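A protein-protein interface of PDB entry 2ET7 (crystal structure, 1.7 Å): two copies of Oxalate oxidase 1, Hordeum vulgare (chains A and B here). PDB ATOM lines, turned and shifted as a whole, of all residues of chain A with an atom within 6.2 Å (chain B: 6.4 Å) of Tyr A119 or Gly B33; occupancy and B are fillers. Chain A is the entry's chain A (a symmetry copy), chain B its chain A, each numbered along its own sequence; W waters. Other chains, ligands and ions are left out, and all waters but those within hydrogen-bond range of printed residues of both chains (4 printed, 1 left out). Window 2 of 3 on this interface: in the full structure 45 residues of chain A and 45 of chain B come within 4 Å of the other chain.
No position is printed for both chains.
Of the 11 printed residues of chain B, 7 touch a printed residue of chain A. Hydrophobic or aromatic side chains of chain B within 4 Å of the printed part of chain A: Phe B9, Phe B36, Leu B37 and Phe B38. Of the 11 printed residues of chain A, 5 touch a printed residue of chain B. Printed residues of chain A that touch a printed residue of chain B: Val A106, Ile A108, Gly A110, Tyr A119 and Arg A121. Along chain A the printed residues that touch a printed residue of chain B span positions 106 to 121. Among the printed residues, Asp or Glu carboxylates within 4 Å of a Lys or Arg side-chain nitrogen of the other chain: Arg A121 with Asp B35 (2.8 Å).
O of Val A106 touches CZ of Phe B38, at 3.8 Å. Leu B37 touches Ile A108 (CD1 to CG2, 3.6 Å). Phe B38 touches Ile A108 (CZ to CD1, 3.7 Å). CA of Gly A110 touches CZ of Phe B9, at 3.95 Å. CE1 of Tyr A119 touches CE1 of Phe B9 (3.6 Å). Tyr A119 touches Gly B33. O of Asp B34 touches CD2 of Tyr A119, 3.5 Å away. Tyr A119 touches Phe B36. Arg A121 touches Phe B38 (CD to CG, 3.4 Å).
Water W3 lies within hydrogen-bond range of the side-chain hydroxyl of Ser A114 (2.7 Å) and the side-chain sulfur of Met B29 (3.7 Å). Water W2 bridges the backbone carbonyl oxygen of Met B29 (2.7 Å) and the side-chain amino group of Lys A117 (2.8 Å). Water W4 lies within hydrogen-bond range of O of Gly B33 and OH of Tyr A119. Water W1 bridges O of Ser B30 and NZ of Lys A117.
The guanidinium group (NH1) of Arg A121 is in salt-bridge range of the side-chain carboxylate (OD1) of Asp B35, 2.8 Å away.
The backbone NH (N) of Val A106 sits at hydrogen-bond distance from the backbone carbonyl oxygen (O) of Arg A121. O of Tyr A119 lies within hydrogen-bond range of N of Ile A108. O of Lys A117 lies within hydrogen-bond range of N of Gly A110 (2.8 Å).
Ser A114 touches none of the printed residues of chain B. Of chain B, only Phe B9 (3.6 Å), Gly B33 (3.6 Å), Asp B34 (3.5 Å) and Phe B36 (3.7 Å) come within 4 Å of Tyr A119. Of the printed residues of chain A, Phe B9 touches Gly A110 and Tyr A119. Glu B31 touches none of the printed residues of chain A. Of chain A, only Tyr A119 comes within 4 Å of Gly B33. Of the printed residues of chain A, Asp B35 touches Arg A121. Printed residues of chain A within 4 Å of Phe B36: Tyr A119. Printed residues of chain A within 4 Å of Phe B38: Val A106, Ile A108 and Arg A121. The nearest printed residue of chain A that does not touch Phe B36 is Arg A121 (7.2 Å).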
ATOM      1  N   VAL A 106      -3.460 -26.883  -5.628  1.00  0.00           N
ATOM      2  CA  VAL A 106      -3.999 -28.248  -5.570  1.00  0.00           C
ATOM      3  C   VAL A 106      -5.438 -28.180  -6.035  1.00  0.00           C
ATOM      4  O   VAL A 106      -6.231 -27.428  -5.457  1.00  0.00           O
ATOM      5  CB  VAL A 106      -3.947 -28.785  -4.105  1.00  0.00           C
ATOM      6  CG1 VAL A 106      -4.581 -30.174  -4.019  1.00  0.00           C
ATOM      7  CG2 VAL A 106      -2.519 -28.823  -3.595  1.00  0.00           C
ATOM      8  N   GLY A 107      -5.770 -28.961  -7.072  1.00  0.00           N
ATOM      9  CA  GLY A 107      -7.129 -28.968  -7.639  1.00  0.00           C
ATOM     10  C   GLY A 107      -7.707 -30.364  -7.583  1.00  0.00           C
ATOM     11  O   GLY A 107      -6.997 -31.352  -7.849  1.00  0.00           O
ATOM     12  N   ILE A 108      -8.978 -30.438  -7.206  1.00  0.00           N
ATOM     13  CA  ILE A 108      -9.683 -31.705  -7.045  1.00  0.00           C
ATOM     14  C   ILE A 108     -11.007 -31.534  -7.790  1.00  0.00           C
ATOM     15  O   ILE A 108     -11.683 -30.508  -7.629  1.00  0.00           O
ATOM     16  CB  ILE A 108      -9.949 -31.986  -5.533  1.00  0.00           C
ATOM     17  CG1 ILE A 108      -8.630 -31.904  -4.754  1.00  0.00           C
ATOM     18  CG2 ILE A 108     -10.647 -33.340  -5.348  1.00  0.00           C
ATOM     19  CD1 ILE A 108      -8.762 -31.493  -3.321  1.00  0.00           C
ATOM     20  N   LEU A 109     -11.379 -32.527  -8.594  1.00  0.00           N
ATOM     21  CA  LEU A 109     -12.529 -32.404  -9.495  1.00  0.00           C
ATOM     22  C   LEU A 109     -13.621 -33.385  -9.113  1.00  0.00           C
ATOM     23  O   LEU A 109     -13.357 -34.581  -9.002  1.00  0.00           O
ATOM     24  CB  LEU A 109     -12.067 -32.652 -10.937  1.00  0.00           C
ATOM     25  CG  LEU A 109     -11.159 -31.521 -11.454  1.00  0.00           C
ATOM     26  CD1 LEU A 109      -9.843 -32.055 -12.009  1.00  0.00           C
ATOM     27  CD2 LEU A 109     -11.916 -30.695 -12.457  1.00  0.00           C
ATOM     28  N   GLY A 110     -14.848 -32.890  -8.907  1.00  0.00           N
ATOM     29  CA  GLY A 110     -16.019 -33.760  -8.775  1.00  0.00           C
ATOM     30  C   GLY A 110     -16.365 -34.519 -10.054  1.00  0.00           C
ATOM     31  O   GLY A 110     -15.919 -34.161 -11.166  1.00  0.00           O
ATOM     32  N   SER A 114     -21.735 -34.344  -9.647  1.00  0.00           N
ATOM     33  CA  SER A 114     -21.282 -33.184  -8.869  1.00  0.00           C
ATOM     34  C   SER A 114     -21.009 -31.974  -9.773  1.00  0.00           C
ATOM     35  O   SER A 114     -20.374 -31.003  -9.352  1.00  0.00           O
ATOM     36  CB  SER A 114     -20.016 -33.541  -8.059  1.00  0.00           C
ATOM     37  OG  SER A 114     -20.277 -34.605  -7.153  1.00  0.00           O
ATOM     38  N   LYS A 117     -17.363 -30.150 -10.668  1.00  0.00           N
ATOM     39  CA  LYS A 117     -16.837 -28.982  -9.964  1.00  0.00           C
ATOM     40  C   LYS A 117     -15.341 -29.105  -9.711  1.00  0.00           C
ATOM     41  O   LYS A 117     -14.856 -30.163  -9.321  1.00  0.00           O
ATOM     42  CB  LYS A 117     -17.555 -28.753  -8.641  1.00  0.00           C
ATOM     43  CG  LYS A 117     -19.000 -28.256  -8.860  1.00  0.00           C
ATOM     44  CD  LYS A 117     -19.767 -28.082  -7.567  1.00  0.00           C
ATOM     45  CE  LYS A 117     -21.250 -27.976  -7.886  1.00  0.00           C
ATOM     46  NZ  LYS A 117     -22.046 -27.721  -6.655  1.00  0.00           N
ATOM     47  N   LEU A 118     -14.636 -27.996  -9.920  1.00  0.00           N
ATOM     48  CA  LEU A 118     -13.218 -27.902  -9.588  1.00  0.00           C
ATOM     49  C   LEU A 118     -13.046 -27.129  -8.291  1.00  0.00           C
ATOM     50  O   LEU A 118     -13.447 -25.960  -8.192  1.00  0.00           O
ATOM     51  CB  LEU A 118     -12.431 -27.196 -10.717  1.00  0.00           C
ATOM     52  CG  LEU A 118     -10.955 -26.855 -10.427  1.00  0.00           C
ATOM     53  CD1 LEU A 118     -10.154 -28.118 -10.046  1.00  0.00           C
ATOM     54  CD2 LEU A 118     -10.317 -26.100 -11.616  1.00  0.00           C
ATOM     55  N   TYR A 119     -12.440 -27.788  -7.310  1.00  0.00           N
ATOM     56  CA  TYR A 119     -12.109 -27.176  -6.034  1.00  0.00           C
ATOM     57  C   TYR A 119     -10.609 -27.004  -6.003  1.00  0.00           C
ATOM     58  O   TYR A 119      -9.873 -27.982  -6.129  1.00  0.00           O
ATOM     59  CB  TYR A 119     -12.504 -28.114  -4.897  1.00  0.00           C
ATOM     60  CG  TYR A 119     -13.957 -28.434  -4.862  1.00  0.00           C
ATOM     61  CD1 TYR A 119     -14.421 -29.682  -5.267  1.00  0.00           C
ATOM     62  CD2 TYR A 119     -14.878 -27.489  -4.418  1.00  0.00           C
ATOM     63  CE1 TYR A 119     -15.794 -29.982  -5.231  1.00  0.00           C
ATOM     64  CE2 TYR A 119     -16.231 -27.772  -4.376  1.00  0.00           C
ATOM     65  CZ  TYR A 119     -16.684 -29.016  -4.784  1.00  0.00           C
ATOM     66  OH  TYR A 119     -18.034 -29.280  -4.724  1.00  0.00           O
ATOM     67  N   SER A 120     -10.141 -25.774  -5.845  1.00  0.00           N
ATOM     68  CA  SER A 120      -8.694 -25.578  -5.831  1.00  0.00           C
ATOM     69  C   SER A 120      -8.272 -24.480  -4.896  1.00  0.00           C
ATOM     70  O   SER A 120      -8.995 -23.502  -4.714  1.00  0.00           O
ATOM     71  CB  SER A 120      -8.152 -25.307  -7.242  1.00  0.00           C
ATOM     72  OG  SER A 120      -8.669 -24.092  -7.796  1.00  0.00           O
ATOM     73  N   ARG A 121      -7.089 -24.624  -4.324  1.00  0.00           N
ATOM     74  CA  ARG A 121      -6.518 -23.547  -3.537  1.00  0.00           C
ATOM     75  C   ARG A 121      -5.007 -23.686  -3.448  1.00  0.00           C
ATOM     76  O   ARG A 121      -4.448 -24.746  -3.734  1.00  0.00           O
ATOM     77  CB  ARG A 121      -7.132 -23.482  -2.133  1.00  0.00           C
ATOM     78  CG  ARG A 121      -6.657 -24.520  -1.170  1.00  0.00           C
ATOM     79  CD  ARG A 121      -7.265 -24.270   0.200  1.00  0.00           C
ATOM     80  NE  ARG A 121      -6.586 -23.235   0.962  1.00  0.00           N
ATOM     81  CZ  ARG A 121      -6.988 -22.798   2.153  1.00  0.00           C
ATOM     82  NH1 ARG A 121      -8.091 -23.289   2.736  1.00  0.00           N
ATOM     83  NH2 ARG A 121      -6.284 -21.856   2.771  1.00  0.00           N
ATOM     84  N   PHE B   9     -18.663 -36.678  -2.298  1.00  0.00           N
ATOM     85  CA  PHE B   9     -18.370 -35.939  -1.058  1.00  0.00           C
ATOM     86  C   PHE B   9     -19.553 -36.039  -0.132  1.00  0.00           C
ATOM     87  O   PHE B   9     -20.693 -36.218  -0.585  1.00  0.00           O
ATOM     88  CB  PHE B   9     -18.105 -34.450  -1.342  1.00  0.00           C
ATOM     89  CG  PHE B   9     -17.244 -34.185  -2.566  1.00  0.00           C
ATOM     90  CD1 PHE B   9     -17.810 -33.629  -3.714  1.00  0.00           C
ATOM     91  CD2 PHE B   9     -15.879 -34.480  -2.561  1.00  0.00           C
ATOM     92  CE1 PHE B   9     -17.026 -33.375  -4.856  1.00  0.00           C
ATOM     93  CE2 PHE B   9     -15.082 -34.222  -3.691  1.00  0.00           C
ATOM     94  CZ  PHE B   9     -15.661 -33.683  -4.838  1.00  0.00           C
ATOM     95  N   MET B  29     -25.113 -31.140   0.221  1.00  0.00           N
ATOM     96  CA  MET B  29     -24.003 -31.006  -0.694  1.00  0.00           C
ATOM     97  C   MET B  29     -24.003 -29.640  -1.338  1.00  0.00           C
ATOM     98  O   MET B  29     -22.945 -29.036  -1.526  1.00  0.00           O
ATOM     99  CB  MET B  29     -24.093 -32.075  -1.788  1.00  0.00           C
ATOM    100  CG  MET B  29     -22.789 -32.351  -2.507  1.00  0.00           C
ATOM    101  SD  MET B  29     -21.419 -32.677  -1.372  1.00  0.00           S
ATOM    102  CE  MET B  29     -20.434 -31.205  -1.590  1.00  0.00           C
ATOM    103  N   SER B  30     -25.204 -29.147  -1.647  1.00  0.00           N
ATOM    104  CA  SER B  30     -25.374 -27.860  -2.303  1.00  0.00           C
ATOM    105  C   SER B  30     -24.724 -26.730  -1.502  1.00  0.00           C
ATOM    106  O   SER B  30     -24.335 -25.715  -2.084  1.00  0.00           O
ATOM    107  CB  SER B  30     -26.861 -27.568  -2.513  1.00  0.00           C
ATOM    108  OG  SER B  30     -27.487 -27.385  -1.258  1.00  0.00           O
ATOM    109  N   GLU B  31     -24.569 -26.934  -0.186  1.00  0.00           N
ATOM    110  CA  GLU B  31     -24.151 -25.883   0.761  1.00  0.00           C
ATOM    111  C   GLU B  31     -22.722 -25.979   1.328  1.00  0.00           C
ATOM    112  O   GLU B  31     -22.372 -25.244   2.256  1.00  0.00           O
ATOM    113  CB  GLU B  31     -25.133 -25.844   1.926  1.00  0.00           C
ATOM    114  CG  GLU B  31     -26.564 -25.485   1.483  1.00  0.00           C
ATOM    115  CD  GLU B  31     -27.601 -25.660   2.575  1.00  0.00           C
ATOM    116  OE1 GLU B  31     -27.230 -25.916   3.745  1.00  0.00           O
ATOM    117  OE2 GLU B  31     -28.811 -25.532   2.255  1.00  0.00           O
ATOM    118  N   ALA B  32     -21.910 -26.871   0.771  1.00  0.00           N
ATOM    119  CA  ALA B  32     -20.590 -27.173   1.338  1.00  0.00           C
ATOM    120  C   ALA B  32     -19.527 -26.113   1.060  1.00  0.00           C
ATOM    121  O   ALA B  32     -18.493 -26.093   1.733  1.00  0.00           O
ATOM    122  CB  ALA B  32     -20.110 -28.514   0.823  1.00  0.00           C
ATOM    123  N   GLY B  33     -19.762 -25.246   0.070  1.00  0.00           N
ATOM    124  CA  GLY B  33     -18.724 -24.286  -0.335  1.00  0.00           C
ATOM    125  C   GLY B  33     -17.601 -24.996  -1.074  1.00  0.00           C
ATOM    126  O   GLY B  33     -17.793 -26.140  -1.532  1.00  0.00           O
ATOM    127  N   ASP B  34     -16.449 -24.321  -1.161  1.00  0.00           N
ATOM    128  CA  ASP B  34     -15.273 -24.723  -1.957  1.00  0.00           C
ATOM    129  C   ASP B  34     -14.148 -25.346  -1.206  1.00  0.00           C
ATOM    130  O   ASP B  34     -13.231 -25.847  -1.854  1.00  0.00           O
ATOM    131  CB  ASP B  34     -14.545 -23.469  -2.456  1.00  0.00           C
ATOM    132  CG  ASP B  34     -15.193 -22.883  -3.575  1.00  0.00           C
ATOM    133  OD1 ASP B  34     -16.031 -23.601  -4.175  1.00  0.00           O
ATOM    134  OD2 ASP B  34     -14.874 -21.719  -3.843  1.00  0.00           O
ATOM    135  N   ASP B  35     -14.156 -25.217   0.123  1.00  0.00           N
ATOM    136  CA  ASP B  35     -12.927 -25.379   0.915  1.00  0.00           C
ATOM    137  C   ASP B  35     -12.896 -26.588   1.835  1.00  0.00           C
ATOM    138  O   ASP B  35     -11.955 -26.725   2.641  1.00  0.00           O
ATOM    139  CB  ASP B  35     -12.681 -24.125   1.762  1.00  0.00           C
ATOM    140  CG  ASP B  35     -11.234 -23.948   2.141  1.00  0.00           C
ATOM    141  OD1 ASP B  35     -10.350 -24.143   1.272  1.00  0.00           O
ATOM    142  OD2 ASP B  35     -10.974 -23.594   3.309  1.00  0.00           O
ATOM    143  N   PHE B  36     -13.915 -27.447   1.721  1.00  0.00           N
ATOM    144  CA  PHE B  36     -14.056 -28.562   2.666  1.00  0.00           C
ATOM    145  C   PHE B  36     -12.978 -29.640   2.517  1.00  0.00           C
ATOM    146  O   PHE B  36     -12.724 -30.399   3.461  1.00  0.00           O
ATOM    147  CB  PHE B  36     -15.469 -29.184   2.570  1.00  0.00           C
ATOM    148  CG  PHE B  36     -15.834 -29.666   1.199  1.00  0.00           C
ATOM    149  CD1 PHE B  36     -15.586 -31.007   0.829  1.00  0.00           C
ATOM    150  CD2 PHE B  36     -16.473 -28.817   0.283  1.00  0.00           C
ATOM    151  CE1 PHE B  36     -15.931 -31.466  -0.450  1.00  0.00           C
ATOM    152  CE2 PHE B  36     -16.824 -29.262  -1.011  1.00  0.00           C
ATOM    153  CZ  PHE B  36     -16.564 -30.606  -1.372  1.00  0.00           C
ATOM    154  N   LEU B  37     -12.360 -29.727   1.338  1.00  0.00           N
ATOM    155  CA  LEU B  37     -11.292 -30.726   1.102  1.00  0.00           C
ATOM    156  C   LEU B  37      -9.912 -30.288   1.612  1.00  0.00           C
ATOM    157  O   LEU B  37      -8.917 -30.998   1.392  1.00  0.00           O
ATOM    158  CB  LEU B  37     -11.199 -31.079  -0.399  1.00  0.00           C
ATOM    159  CG  LEU B  37     -12.440 -31.725  -1.039  1.00  0.00           C
ATOM    160  CD1 LEU B  37     -12.330 -31.807  -2.558  1.00  0.00           C
ATOM    161  CD2 LEU B  37     -12.686 -33.118  -0.432  1.00  0.00           C
ATOM    162  N   PHE B  38      -9.846 -29.121   2.266  1.00  0.00           N
ATOM    163  CA  PHE B  38      -8.574 -28.525   2.737  1.00  0.00           C
ATOM    164  C   PHE B  38      -8.583 -28.201   4.225  1.00  0.00           C
ATOM    165  O   PHE B  38      -9.633 -27.883   4.785  1.00  0.00           O
ATOM    166  CB  PHE B  38      -8.280 -27.257   1.943  1.00  0.00           C
ATOM    167  CG  PHE B  38      -8.250 -27.484   0.465  1.00  0.00           C
ATOM    168  CD1 PHE B  38      -9.380 -27.232  -0.314  1.00  0.00           C
ATOM    169  CD2 PHE B  38      -7.099 -27.989  -0.151  1.00  0.00           C
ATOM    170  CE1 PHE B  38      -9.379 -27.468  -1.691  1.00  0.00           C
ATOM    171  CE2 PHE B  38      -7.069 -28.227  -1.527  1.00  0.00           C
ATOM    172  CZ  PHE B  38      -8.217 -27.970  -2.305  1.00  0.00           C
HETATM  173  O   HOH W   1     -23.766 -25.905  -4.824  1.00  0.00           O
HETATM  174  O   HOH W   2     -22.033 -28.078  -3.894  1.00  0.00           O
HETATM  175  O   HOH W   3     -21.263 -33.263  -5.035  1.00  0.00           O
HETATM  176  O   HOH W   4     -19.546 -27.134  -3.472  1.00  0.00           O
